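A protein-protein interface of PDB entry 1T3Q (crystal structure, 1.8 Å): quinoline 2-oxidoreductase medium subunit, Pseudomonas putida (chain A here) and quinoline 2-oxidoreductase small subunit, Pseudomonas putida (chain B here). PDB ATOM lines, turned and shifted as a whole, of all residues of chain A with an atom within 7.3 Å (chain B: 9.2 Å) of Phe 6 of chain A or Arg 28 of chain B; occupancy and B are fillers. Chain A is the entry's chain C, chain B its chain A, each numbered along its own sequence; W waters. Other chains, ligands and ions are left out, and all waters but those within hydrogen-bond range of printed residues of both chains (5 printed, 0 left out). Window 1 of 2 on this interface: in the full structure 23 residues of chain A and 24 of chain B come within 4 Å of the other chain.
The side-chain carboxylate (OD1) of Asp 33 of chain B is in salt-bridge range of the side-chain amino group (NZ) of Lys 2 of chain A.
The side-chain carboxylate (OE1) of Glu 49 of chain B lies within salt-bridge range of the side-chain amino group (NZ) of Lys 2 of chain A, at 2.8 Å.
NH1 of Arg 28 of chain B sits close to NH2 of Arg 43 of chain A (3.3 Å).
The guanidinium group (NH1) of Arg 28 of chain B lies within hydrogen-bond range of the backbone carbonyl oxygen (O) of Phe 3 of chain A, at 2.9 Å.
NE of Arg 43 of chain A lies within hydrogen-bond range of O of Lys 2 of chain A (2.8 Å).
N of Asp 33 of chain B sits at hydrogen-bond distance from ND1 of His 30 of chain B.
The backbone carbonyl oxygen (O) of Arg 43 of chain A is in hydrogen-bond range of the side-chain hydroxyl (OH) of Tyr 46 of chain A (3.0 Å).
OE1 of Glu 49 of chain B lies within hydrogen-bond range of NE2 of His 30 of chain B (2.9 Å).
N of Leu 31 of chain B sits at hydrogen-bond distance from O of Thr 70 of chain B (2.7 Å).
NH2 of Arg 43 of chain A sits at hydrogen-bond distance from O of Phe 3 of chain A (3.5 Å).
CE1 of Phe 3 of chain A touches CB of His 30 of chain B, at 3.9 Å.
Phe 3 of chain A touches Leu 71 of chain B (CE1 to CD2, 3.8 Å).
Pro 27 of chain B touches Phe 6 of chain A (CB to O, 3.3 Å).
CZ of Phe 6 of chain A touches CD2 of Leu 71 of chain B (3.99 Å).
Tyr 8 of chain A touches Met 10 of chain B (CD2 to CE, 3.97 Å).
CB of Pro 27 of chain B touches CB of Tyr 8 of chain A, at 3.8 Å.
CD1 of Tyr 8 of chain A touches CD1 of Leu 71 of chain B (3.99 Å).
Ile 30 of chain A touches Gln 74 of chain B (CD1 to NE2, 3.6 Å).
CD1 of Leu 37 of chain A touches N of Thr 70 of chain B (3.7 Å).
Leu 71 of chain B touches Leu 37 of chain A (CD2 to CD2, 3.9 Å).
Pro 4 of chain A touches one residue of chain B.
Of chain B, only Arg 28 comes within 4 Å of Ala 5 of chain A.
Of the printed residues of chain B, Tyr 8 of chain A touches Met 10, Pro 27, Leu 71, Val 73 and Gln 74.
Of the printed residues of chain B, Arg 43 of chain A touches Arg 28.
The nearest residue of chain A that does not touch Arg 28 of chain B is Lys 2 of chain A (5.1 Å).
The nearest printed residue of chain A that does not touch Leu 71 of chain B is Leu 50 of chain A (4.1 Å).
Of the 19 printed residues of chain B, 11 touch a printed residue of chain A.
Hydrophobic or aromatic side chains of chain B that line the printed part of chain A: Met 10, Pro 27, His 30, Leu 71 and Val 73.
Along chain B the printed residues that touch a printed residue of chain A span positions 10 to 74.
Of the 17 printed residues of chain A, 9 touch a printed residue of chain B.
Printed residues of chain A that touch a printed residue of chain B: Lys 2, Phe 3, Pro 4, Ala 5, Phe 6, Tyr 8, Ile 30, Leu 37 and Arg 43.
Hydrophobic or aromatic side chains of chain A within 4 Å of the printed part of chain B: Phe 3, Ala 5, Phe 6, Tyr 8, Ile 30 and Leu 37.
Water W2 bridges O of Arg 28 of chain B (2.6 Å) and O of Phe 3 of chain A (2.7 Å).
Water W3 bridges the side-chain hydroxyl (OH) of Tyr 8 of chain A (2.7 Å) and the backbone carbonyl oxygen (O) of Val 73 of chain B (3.2 Å).
Water W5 bridges N of Tyr 8 of chain A (2.9 Å) and SD of Met 10 of chain B (3.6 Å).
Water W4 lies within hydrogen-bond range of the backbone NH of Phe 3 of chain A (2.9 Å) and the backbone carbonyl oxygen of Arg 28 of chain B (3.4 Å).
Water W1 lies within hydrogen-bond range of O of Phe 6 of chain A (2.9 Å) and N of Arg 28 of chain B (3.0 Å).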
ATOM      1  N   LYS A   2      18.557  18.783 -13.184  1.00  0.00           N
ATOM      2  CA  LYS A   2      17.146  19.096 -13.376  1.00  0.00           C
ATOM      3  C   LYS A   2      16.818  18.669 -14.811  1.00  0.00           C
ATOM      4  O   LYS A   2      17.653  18.813 -15.711  1.00  0.00           O
ATOM      5  CB  LYS A   2      16.881  20.596 -13.201  1.00  0.00           C
ATOM      6  CG  LYS A   2      17.183  21.146 -11.809  1.00  0.00           C
ATOM      7  CD  LYS A   2      16.441  20.390 -10.719  1.00  0.00           C
ATOM      8  CE  LYS A   2      16.747  20.969  -9.341  1.00  0.00           C
ATOM      9  NZ  LYS A   2      16.024  20.252  -8.249  1.00  0.00           N
ATOM     10  N   PHE A   3      15.621  18.132 -15.021  1.00  0.00           N
ATOM     11  CA  PHE A   3      15.216  17.681 -16.351  1.00  0.00           C
ATOM     12  C   PHE A   3      15.275  18.814 -17.368  1.00  0.00           C
ATOM     13  O   PHE A   3      15.158  19.985 -17.013  1.00  0.00           O
ATOM     14  CB  PHE A   3      13.764  17.187 -16.355  1.00  0.00           C
ATOM     15  CG  PHE A   3      13.436  16.204 -15.273  1.00  0.00           C
ATOM     16  CD1 PHE A   3      12.133  16.122 -14.783  1.00  0.00           C
ATOM     17  CD2 PHE A   3      14.404  15.353 -14.751  1.00  0.00           C
ATOM     18  CE1 PHE A   3      11.802  15.213 -13.790  1.00  0.00           C
ATOM     19  CE2 PHE A   3      14.079  14.434 -13.753  1.00  0.00           C
ATOM     20  CZ  PHE A   3      12.779  14.366 -13.274  1.00  0.00           C
ATOM     21  N   PRO A   4      15.484  18.475 -18.648  1.00  0.00           N
ATOM     22  CA  PRO A   4      15.516  19.529 -19.662  1.00  0.00           C
ATOM     23  C   PRO A   4      14.030  19.832 -19.883  1.00  0.00           C
ATOM     24  O   PRO A   4      13.177  19.072 -19.417  1.00  0.00           O
ATOM     25  CB  PRO A   4      16.180  18.842 -20.856  1.00  0.00           C
ATOM     26  CG  PRO A   4      15.776  17.420 -20.698  1.00  0.00           C
ATOM     27  CD  PRO A   4      15.911  17.181 -19.212  1.00  0.00           C
ATOM     28  N   ALA A   5      13.709  20.921 -20.570  1.00  0.00           N
ATOM     29  CA  ALA A   5      12.309  21.286 -20.786  1.00  0.00           C
ATOM     30  C   ALA A   5      11.563  20.408 -21.794  1.00  0.00           C
ATOM     31  O   ALA A   5      12.160  19.854 -22.712  1.00  0.00           O
ATOM     32  CB  ALA A   5      12.220  22.747 -21.207  1.00  0.00           C
ATOM     33  N   PHE A   6      10.250  20.283 -21.602  1.00  0.00           N
ATOM     34  CA  PHE A   6       9.397  19.502 -22.498  1.00  0.00           C
ATOM     35  C   PHE A   6       7.921  19.745 -22.193  1.00  0.00           C
ATOM     36  O   PHE A   6       7.572  20.187 -21.098  1.00  0.00           O
ATOM     37  CB  PHE A   6       9.717  18.001 -22.385  1.00  0.00           C
ATOM     38  CG  PHE A   6       9.681  17.467 -20.974  1.00  0.00           C
ATOM     39  CD1 PHE A   6       8.470  17.231 -20.329  1.00  0.00           C
ATOM     40  CD2 PHE A   6      10.867  17.229 -20.280  1.00  0.00           C
ATOM     41  CE1 PHE A   6       8.441  16.768 -19.009  1.00  0.00           C
ATOM     42  CE2 PHE A   6      10.848  16.766 -18.966  1.00  0.00           C
ATOM     43  CZ  PHE A   6       9.631  16.535 -18.328  1.00  0.00           C
ATOM     44  N   SER A   7       7.055  19.483 -23.169  1.00  0.00           N
ATOM     45  CA  SER A   7       5.622  19.653 -22.957  1.00  0.00           C
ATOM     46  C   SER A   7       5.084  18.318 -22.454  1.00  0.00           C
ATOM     47  O   SER A   7       5.808  17.322 -22.429  1.00  0.00           O
ATOM     48  CB  SER A   7       4.922  20.062 -24.258  1.00  0.00           C
ATOM     49  OG  SER A   7       5.111  19.080 -25.254  1.00  0.00           O
ATOM     50  N   TYR A   8       3.815  18.290 -22.063  1.00  0.00           N
ATOM     51  CA  TYR A   8       3.220  17.073 -21.521  1.00  0.00           C
ATOM     52  C   TYR A   8       1.779  16.861 -21.958  1.00  0.00           C
ATOM     53  O   TYR A   8       0.993  17.804 -22.014  1.00  0.00           O
ATOM     54  CB  TYR A   8       3.279  17.130 -19.994  1.00  0.00           C
ATOM     55  CG  TYR A   8       2.571  16.005 -19.273  1.00  0.00           C
ATOM     56  CD1 TYR A   8       3.225  14.801 -18.992  1.00  0.00           C
ATOM     57  CD2 TYR A   8       1.258  16.162 -18.824  1.00  0.00           C
ATOM     58  CE1 TYR A   8       2.588  13.784 -18.271  1.00  0.00           C
ATOM     59  CE2 TYR A   8       0.614  15.155 -18.108  1.00  0.00           C
ATOM     60  CZ  TYR A   8       1.284  13.971 -17.834  1.00  0.00           C
ATOM     61  OH  TYR A   8       0.647  12.987 -17.112  1.00  0.00           O
ATOM     62  N   ILE A  30       5.932   8.222 -21.500  1.00  0.00           N
ATOM     63  CA  ILE A  30       6.310   8.100 -20.103  1.00  0.00           C
ATOM     64  C   ILE A  30       5.235   7.244 -19.447  1.00  0.00           C
ATOM     65  O   ILE A  30       4.041   7.453 -19.664  1.00  0.00           O
ATOM     66  CB  ILE A  30       6.422   9.457 -19.344  1.00  0.00           C
ATOM     67  CG1 ILE A  30       6.862   9.171 -17.898  1.00  0.00           C
ATOM     68  CG2 ILE A  30       5.094  10.202 -19.342  1.00  0.00           C
ATOM     69  CD1 ILE A  30       7.092  10.407 -17.035  1.00  0.00           C
ATOM     70  N   LEU A  37      12.941   9.259 -16.082  1.00  0.00           N
ATOM     71  CA  LEU A  37      13.276  10.473 -15.349  1.00  0.00           C
ATOM     72  C   LEU A  37      14.742  10.477 -14.918  1.00  0.00           C
ATOM     73  O   LEU A  37      15.395  11.520 -14.955  1.00  0.00           O
ATOM     74  CB  LEU A  37      12.330  10.670 -14.153  1.00  0.00           C
ATOM     75  CG  LEU A  37      10.841  10.837 -14.500  1.00  0.00           C
ATOM     76  CD1 LEU A  37      10.123  11.552 -13.356  1.00  0.00           C
ATOM     77  CD2 LEU A  37      10.670  11.634 -15.781  1.00  0.00           C
ATOM     78  N   LEU A  40      16.529  11.685 -17.750  1.00  0.00           N
ATOM     79  CA  LEU A  40      16.274  13.108 -17.947  1.00  0.00           C
ATOM     80  C   LEU A  40      17.079  13.926 -16.947  1.00  0.00           C
ATOM     81  O   LEU A  40      17.567  15.010 -17.270  1.00  0.00           O
ATOM     82  CB  LEU A  40      14.780  13.414 -17.779  1.00  0.00           C
ATOM     83  CG  LEU A  40      13.864  13.015 -18.941  1.00  0.00           C
ATOM     84  CD1 LEU A  40      12.408  13.172 -18.534  1.00  0.00           C
ATOM     85  CD2 LEU A  40      14.173  13.889 -20.148  1.00  0.00           C
ATOM     86  N   ARG A  43      20.205  14.371 -18.178  1.00  0.00           N
ATOM     87  CA  ARG A  43      20.094  15.003 -19.480  1.00  0.00           C
ATOM     88  C   ARG A  43      20.718  14.143 -20.567  1.00  0.00           C
ATOM     89  O   ARG A  43      21.484  14.627 -21.403  1.00  0.00           O
ATOM     90  CB  ARG A  43      20.731  16.397 -19.447  1.00  0.00           C
ATOM     91  CG  ARG A  43      20.065  17.299 -18.421  1.00  0.00           C
ATOM     92  CD  ARG A  43      20.230  18.777 -18.718  1.00  0.00           C
ATOM     93  NE  ARG A  43      19.394  19.565 -17.816  1.00  0.00           N
ATOM     94  CZ  ARG A  43      19.075  20.840 -18.000  1.00  0.00           C
ATOM     95  NH1 ARG A  43      19.519  21.500 -19.065  1.00  0.00           N
ATOM     96  NH2 ARG A  43      18.295  21.457 -17.121  1.00  0.00           N
ATOM     97  N   VAL A  45      18.702  12.347 -22.512  1.00  0.00           N
ATOM     98  CA  VAL A  45      17.681  12.349 -23.556  1.00  0.00           C
ATOM     99  C   VAL A  45      17.020  13.715 -23.528  1.00  0.00           C
ATOM    100  O   VAL A  45      16.922  14.342 -22.470  1.00  0.00           O
ATOM    101  CB  VAL A  45      16.596  11.252 -23.344  1.00  0.00           C
ATOM    102  CG1 VAL A  45      17.236   9.868 -23.385  1.00  0.00           C
ATOM    103  CG2 VAL A  45      15.871  11.468 -22.027  1.00  0.00           C
ATOM    104  N   TYR A  46      16.574  14.182 -24.690  1.00  0.00           N
ATOM    105  CA  TYR A  46      15.945  15.488 -24.779  1.00  0.00           C
ATOM    106  C   TYR A  46      14.626  15.434 -25.533  1.00  0.00           C
ATOM    107  O   TYR A  46      14.532  15.883 -26.673  1.00  0.00           O
ATOM    108  CB  TYR A  46      16.883  16.480 -25.469  1.00  0.00           C
ATOM    109  CG  TYR A  46      18.203  16.677 -24.761  1.00  0.00           C
ATOM    110  CD1 TYR A  46      19.241  15.760 -24.905  1.00  0.00           C
ATOM    111  CD2 TYR A  46      18.411  17.786 -23.940  1.00  0.00           C
ATOM    112  CE1 TYR A  46      20.463  15.942 -24.248  1.00  0.00           C
ATOM    113  CE2 TYR A  46      19.625  17.977 -23.277  1.00  0.00           C
ATOM    114  CZ  TYR A  46      20.645  17.053 -23.436  1.00  0.00           C
ATOM    115  OH  TYR A  46      21.848  17.250 -22.793  1.00  0.00           O
ATOM    116  N   PRO A  47      13.582  14.884 -24.901  1.00  0.00           N
ATOM    117  CA  PRO A  47      12.283  14.805 -25.571  1.00  0.00           C
ATOM    118  C   PRO A  47      11.653  16.180 -25.713  1.00  0.00           C
ATOM    119  O   PRO A  47      11.913  17.081 -24.917  1.00  0.00           O
ATOM    120  CB  PRO A  47      11.479  13.896 -24.650  1.00  0.00           C
ATOM    121  CG  PRO A  47      12.021  14.257 -23.287  1.00  0.00           C
ATOM    122  CD  PRO A  47      13.518  14.311 -23.543  1.00  0.00           C
ATOM    123  N   SER A  48      10.822  16.345 -26.733  1.00  0.00           N
ATOM    124  CA  SER A  48      10.148  17.612 -26.949  1.00  0.00           C
ATOM    125  C   SER A  48       8.888  17.600 -26.100  1.00  0.00           C
ATOM    126  O   SER A  48       8.450  18.629 -25.586  1.00  0.00           O
ATOM    127  CB  SER A  48       9.762  17.749 -28.422  1.00  0.00           C
ATOM    128  OG  SER A  48       8.975  16.641 -28.821  1.00  0.00           O
ATOM    129  N   CYS A  49       8.324  16.406 -25.945  1.00  0.00           N
ATOM    130  CA  CYS A  49       7.087  16.230 -25.205  1.00  0.00           C
ATOM    131  C   CYS A  49       7.012  14.825 -24.620  1.00  0.00           C
ATOM    132  O   CYS A  49       7.477  13.866 -25.231  1.00  0.00           O
ATOM    133  CB  CYS A  49       5.906  16.457 -26.159  1.00  0.00           C
ATOM    134  SG  CYS A  49       4.265  15.987 -25.530  1.00  0.00           S
ATOM    135  N   LEU A  50       6.451  14.707 -23.424  1.00  0.00           N
ATOM    136  CA  LEU A  50       6.295  13.395 -22.814  1.00  0.00           C
ATOM    137  C   LEU A  50       4.821  13.043 -22.892  1.00  0.00           C
ATOM    138  O   LEU A  50       3.962  13.823 -22.480  1.00  0.00           O
ATOM    139  CB  LEU A  50       6.761  13.393 -21.357  1.00  0.00           C
ATOM    140  CG  LEU A  50       8.272  13.543 -21.139  1.00  0.00           C
ATOM    141  CD1 LEU A  50       8.591  13.310 -19.670  1.00  0.00           C
ATOM    142  CD2 LEU A  50       9.026  12.542 -22.008  1.00  0.00           C
ATOM    143  N   GLN B   8       3.460  28.145 -20.039  1.00  0.00           N
ATOM    144  CA  GLN B   8       4.095  26.856 -20.141  1.00  0.00           C
ATOM    145  C   GLN B   8       3.746  26.120 -18.844  1.00  0.00           C
ATOM    146  O   GLN B   8       4.133  24.964 -18.651  1.00  0.00           O
ATOM    147  CB  GLN B   8       5.608  27.021 -20.298  1.00  0.00           C
ATOM    148  CG  GLN B   8       5.944  27.978 -21.428  1.00  0.00           C
ATOM    149  CD  GLN B   8       7.408  28.310 -21.497  1.00  0.00           C
ATOM    150  OE1 GLN B   8       8.170  27.665 -22.216  1.00  0.00           O
ATOM    151  NE2 GLN B   8       7.814  29.327 -20.746  1.00  0.00           N
ATOM    152  N   LEU B   9       2.984  26.800 -17.977  1.00  0.00           N
ATOM    153  CA  LEU B   9       2.531  26.270 -16.676  1.00  0.00           C
ATOM    154  C   LEU B   9       1.196  25.545 -16.768  1.00  0.00           C
ATOM    155  O   LEU B   9       0.253  26.025 -17.401  1.00  0.00           O
ATOM    156  CB  LEU B   9       2.374  27.399 -15.642  1.00  0.00           C
ATOM    157  CG  LEU B   9       3.428  27.624 -14.543  1.00  0.00           C
ATOM    158  CD1 LEU B   9       4.817  27.439 -15.112  1.00  0.00           C
ATOM    159  CD2 LEU B   9       3.274  29.024 -13.947  1.00  0.00           C
ATOM    160  N   MET B  10       1.112  24.405 -16.099  1.00  0.00           N
ATOM    161  CA  MET B  10      -0.100  23.600 -16.090  1.00  0.00           C
ATOM    162  C   MET B  10      -0.781  23.616 -14.722  1.00  0.00           C
ATOM    163  O   MET B  10      -0.121  23.522 -13.683  1.00  0.00           O
ATOM    164  CB  MET B  10       0.233  22.162 -16.496  1.00  0.00           C
ATOM    165  CG  MET B  10       0.667  22.021 -17.950  1.00  0.00           C
ATOM    166  SD  MET B  10       1.006  20.315 -18.408  1.00  0.00           S
ATOM    167  CE  MET B  10      -0.650  19.614 -18.351  1.00  0.00           C
ATOM    168  N   VAL B  25       2.580  24.373 -12.345  1.00  0.00           N
ATOM    169  CA  VAL B  25       3.938  23.903 -12.551  1.00  0.00           C
ATOM    170  C   VAL B  25       4.236  23.614 -14.011  1.00  0.00           C
ATOM    171  O   VAL B  25       3.324  23.446 -14.827  1.00  0.00           O
ATOM    172  CB  VAL B  25       4.195  22.594 -11.760  1.00  0.00           C
ATOM    173  CG1 VAL B  25       4.137  22.863 -10.270  1.00  0.00           C
ATOM    174  CG2 VAL B  25       3.161  21.540 -12.151  1.00  0.00           C
ATOM    175  N   GLU B  26       5.523  23.563 -14.335  1.00  0.00           N
ATOM    176  CA  GLU B  26       5.954  23.229 -15.685  1.00  0.00           C
ATOM    177  C   GLU B  26       6.158  21.721 -15.670  1.00  0.00           C
ATOM    178  O   GLU B  26       6.481  21.148 -14.628  1.00  0.00           O
ATOM    179  CB  GLU B  26       7.282  23.898 -16.028  1.00  0.00           C
ATOM    180  CG  GLU B  26       7.248  25.405 -16.065  1.00  0.00           C
ATOM    181  CD  GLU B  26       8.564  25.988 -16.528  1.00  0.00           C
ATOM    182  OE1 GLU B  26       9.585  25.777 -15.846  1.00  0.00           O
ATOM    183  OE2 GLU B  26       8.580  26.653 -17.583  1.00  0.00           O
ATOM    184  N   PRO B  27       5.976  21.057 -16.821  1.00  0.00           N
ATOM    185  CA  PRO B  27       6.158  19.604 -16.889  1.00  0.00           C
ATOM    186  C   PRO B  27       7.562  19.160 -16.459  1.00  0.00           C
ATOM    187  O   PRO B  27       7.730  18.077 -15.905  1.00  0.00           O
ATOM    188  CB  PRO B  27       5.883  19.293 -18.361  1.00  0.00           C
ATOM    189  CG  PRO B  27       4.874  20.344 -18.741  1.00  0.00           C
ATOM    190  CD  PRO B  27       5.443  21.584 -18.091  1.00  0.00           C
ATOM    191  N   ARG B  28       8.558  20.010 -16.708  1.00  0.00           N
ATOM    192  CA  ARG B  28       9.955  19.708 -16.379  1.00  0.00           C
ATOM    193  C   ARG B  28      10.294  19.646 -14.893  1.00  0.00           C
ATOM    194  O   ARG B  28      11.413  19.279 -14.531  1.00  0.00           O
ATOM    195  CB  ARG B  28      10.889  20.732 -17.040  1.00  0.00           C
ATOM    196  CG  ARG B  28      10.839  22.123 -16.403  1.00  0.00           C
ATOM    197  CD  ARG B  28      11.761  23.109 -17.123  1.00  0.00           C
ATOM    198  NE  ARG B  28      13.133  22.613 -17.225  1.00  0.00           N
ATOM    199  CZ  ARG B  28      14.118  23.255 -17.852  1.00  0.00           C
ATOM    200  NH1 ARG B  28      15.336  22.732 -17.898  1.00  0.00           N
ATOM    201  NH2 ARG B  28      13.887  24.424 -18.433  1.00  0.00           N
ATOM    202  N   MET B  29       9.352  20.013 -14.034  1.00  0.00           N
ATOM    203  CA  MET B  29       9.601  20.002 -12.596  1.00  0.00           C
ATOM    204  C   MET B  29       9.072  18.723 -11.948  1.00  0.00           C
ATOM    205  O   MET B  29       7.914  18.346 -12.169  1.00  0.00           O
ATOM    206  CB  MET B  29       8.936  21.227 -11.944  1.00  0.00           C
ATOM    207  CG  MET B  29       9.114  21.314 -10.430  1.00  0.00           C
ATOM    208  SD  MET B  29       8.403  22.789  -9.672  1.00  0.00           S
ATOM    209  CE  MET B  29       9.770  23.929  -9.798  1.00  0.00           C
ATOM    210  N   HIS B  30       9.907  18.042 -11.162  1.00  0.00           N
ATOM    211  CA  HIS B  30       9.410  16.842 -10.504  1.00  0.00           C
ATOM    212  C   HIS B  30       8.584  17.216  -9.276  1.00  0.00           C
ATOM    213  O   HIS B  30       8.606  18.362  -8.820  1.00  0.00           O
ATOM    214  CB  HIS B  30      10.537  15.845 -10.160  1.00  0.00           C
ATOM    215  CG  HIS B  30      11.717  16.432  -9.440  1.00  0.00           C
ATOM    216  ND1 HIS B  30      11.607  17.109  -8.243  1.00  0.00           N
ATOM    217  CD2 HIS B  30      13.044  16.346  -9.700  1.00  0.00           C
ATOM    218  CE1 HIS B  30      12.814  17.408  -7.796  1.00  0.00           C
ATOM    219  NE2 HIS B  30      13.705  16.955  -8.661  1.00  0.00           N
ATOM    220  N   LEU B  31       7.824  16.252  -8.769  1.00  0.00           N
ATOM    221  CA  LEU B  31       6.946  16.468  -7.626  1.00  0.00           C
ATOM    222  C   LEU B  31       7.652  16.944  -6.361  1.00  0.00           C
ATOM    223  O   LEU B  31       7.121  17.787  -5.629  1.00  0.00           O
ATOM    224  CB  LEU B  31       6.154  15.186  -7.343  1.00  0.00           C
ATOM    225  CG  LEU B  31       5.084  15.263  -6.251  1.00  0.00           C
ATOM    226  CD1 LEU B  31       4.161  16.445  -6.507  1.00  0.00           C
ATOM    227  CD2 LEU B  31       4.302  13.958  -6.223  1.00  0.00           C
ATOM    228  N   ASP B  33      10.339  18.839  -6.080  1.00  0.00           N
ATOM    229  CA  ASP B  33      10.574  20.279  -6.221  1.00  0.00           C
ATOM    230  C   ASP B  33       9.271  21.086  -6.146  1.00  0.00           C
ATOM    231  O   ASP B  33       9.239  22.163  -5.553  1.00  0.00           O
ATOM    232  CB  ASP B  33      11.277  20.588  -7.553  1.00  0.00           C
ATOM    233  CG  ASP B  33      12.795  20.433  -7.479  1.00  0.00           C
ATOM    234  OD1 ASP B  33      13.458  20.569  -8.534  1.00  0.00           O
ATOM    235  OD2 ASP B  33      13.334  20.177  -6.378  1.00  0.00           O
ATOM    236  N   ALA B  34       8.198  20.579  -6.747  1.00  0.00           N
ATOM    237  CA  ALA B  34       6.928  21.303  -6.722  1.00  0.00           C
ATOM    238  C   ALA B  34       6.396  21.428  -5.300  1.00  0.00           C
ATOM    239  O   ALA B  34       5.972  22.509  -4.881  1.00  0.00           O
ATOM    240  CB  ALA B  34       5.901  20.611  -7.616  1.00  0.00           C
ATOM    241  N   GLU B  49      17.927  12.575  -6.421  1.00  0.00           N
ATOM    242  CA  GLU B  49      17.127  12.795  -7.630  1.00  0.00           C
ATOM    243  C   GLU B  49      17.290  11.672  -8.657  1.00  0.00           C
ATOM    244  O   GLU B  49      17.109  11.879  -9.864  1.00  0.00           O
ATOM    245  CB  GLU B  49      17.475  14.157  -8.257  1.00  0.00           C
ATOM    246  CG  GLU B  49      16.932  15.333  -7.446  1.00  0.00           C
ATOM    247  CD  GLU B  49      17.387  16.700  -7.941  1.00  0.00           C
ATOM    248  OE1 GLU B  49      16.515  17.524  -8.292  1.00  0.00           O
ATOM    249  OE2 GLU B  49      18.610  16.956  -7.966  1.00  0.00           O
ATOM    250  N   CYS B  68      10.891  12.482  -6.494  1.00  0.00           N
ATOM    251  CA  CYS B  68      11.866  13.047  -7.425  1.00  0.00           C
ATOM    252  C   CYS B  68      11.741  12.350  -8.782  1.00  0.00           C
ATOM    253  O   CYS B  68      12.239  12.849  -9.796  1.00  0.00           O
ATOM    254  CB  CYS B  68      13.292  12.880  -6.893  1.00  0.00           C
ATOM    255  SG  CYS B  68      13.927  11.211  -6.925  1.00  0.00           S
ATOM    256  N   THR B  70       8.683  11.446  -9.995  1.00  0.00           N
ATOM    257  CA  THR B  70       7.277  11.623 -10.341  1.00  0.00           C
ATOM    258  C   THR B  70       7.173  13.052 -10.853  1.00  0.00           C
ATOM    259  O   THR B  70       7.608  13.974 -10.174  1.00  0.00           O
ATOM    260  CB  THR B  70       6.347  11.490  -9.107  1.00  0.00           C
ATOM    261  OG1 THR B  70       6.494  10.191  -8.517  1.00  0.00           O
ATOM    262  CG2 THR B  70       4.887  11.694  -9.524  1.00  0.00           C
ATOM    263  N   LEU B  71       6.627  13.257 -12.050  1.00  0.00           N
ATOM    264  CA  LEU B  71       6.499  14.626 -12.540  1.00  0.00           C
ATOM    265  C   LEU B  71       5.449  15.305 -11.671  1.00  0.00           C
ATOM    266  O   LEU B  71       4.478  14.668 -11.244  1.00  0.00           O
ATOM    267  CB  LEU B  71       6.040  14.657 -14.008  1.00  0.00           C
ATOM    268  CG  LEU B  71       6.905  14.001 -15.091  1.00  0.00           C
ATOM    269  CD1 LEU B  71       6.248  14.213 -16.450  1.00  0.00           C
ATOM    270  CD2 LEU B  71       8.305  14.610 -15.095  1.00  0.00           C
ATOM    271  N   ALA B  72       5.634  16.590 -11.399  1.00  0.00           N
ATOM    272  CA  ALA B  72       4.663  17.307 -10.593  1.00  0.00           C
ATOM    273  C   ALA B  72       3.302  17.221 -11.280  1.00  0.00           C
ATOM    274  O   ALA B  72       2.274  17.095 -10.616  1.00  0.00           O
ATOM    275  CB  ALA B  72       5.088  18.770 -10.427  1.00  0.00           C
ATOM    276  N   VAL B  73       3.289  17.276 -12.611  1.00  0.00           N
ATOM    277  CA  VAL B  73       2.021  17.199 -13.329  1.00  0.00           C
ATOM    278  C   VAL B  73       1.341  15.835 -13.180  1.00  0.00           C
ATOM    279  O   VAL B  73       0.143  15.708 -13.422  1.00  0.00           O
ATOM    280  CB  VAL B  73       2.173  17.540 -14.841  1.00  0.00           C
ATOM    281  CG1 VAL B  73       2.618  18.981 -14.999  1.00  0.00           C
ATOM    282  CG2 VAL B  73       3.151  16.591 -15.517  1.00  0.00           C
ATOM    283  N   GLN B  74       2.092  14.819 -12.765  1.00  0.00           N
ATOM    284  CA  GLN B  74       1.503  13.495 -12.580  1.00  0.00           C
ATOM    285  C   GLN B  74       0.794  13.377 -11.236  1.00  0.00           C
ATOM    286  O   GLN B  74       0.289  12.314 -10.883  1.00  0.00           O
ATOM    287  CB  GLN B  74       2.567  12.404 -12.717  1.00  0.00           C
ATOM    288  CG  GLN B  74       3.073  12.257 -14.146  1.00  0.00           C
ATOM    289  CD  GLN B  74       4.178  11.235 -14.286  1.00  0.00           C
ATOM    290  OE1 GLN B  74       5.196  11.310 -13.605  1.00  0.00           O
ATOM    291  NE2 GLN B  74       3.987  10.275 -15.181  1.00  0.00           N
HETATM  292  O   HOH W   1       8.735  21.902 -19.006  1.00  0.00           O
HETATM  293  O   HOH W   2      13.566  20.695 -14.958  1.00  0.00           O
HETATM  294  O   HOH W   3      -1.383  13.685 -15.439  1.00  0.00           O
HETATM  295  O   HOH W   4      13.925  17.873 -12.672  1.00  0.00           O
HETATM  296  O   HOH W   5       2.387  20.756 -21.684  1.00  0.00           O
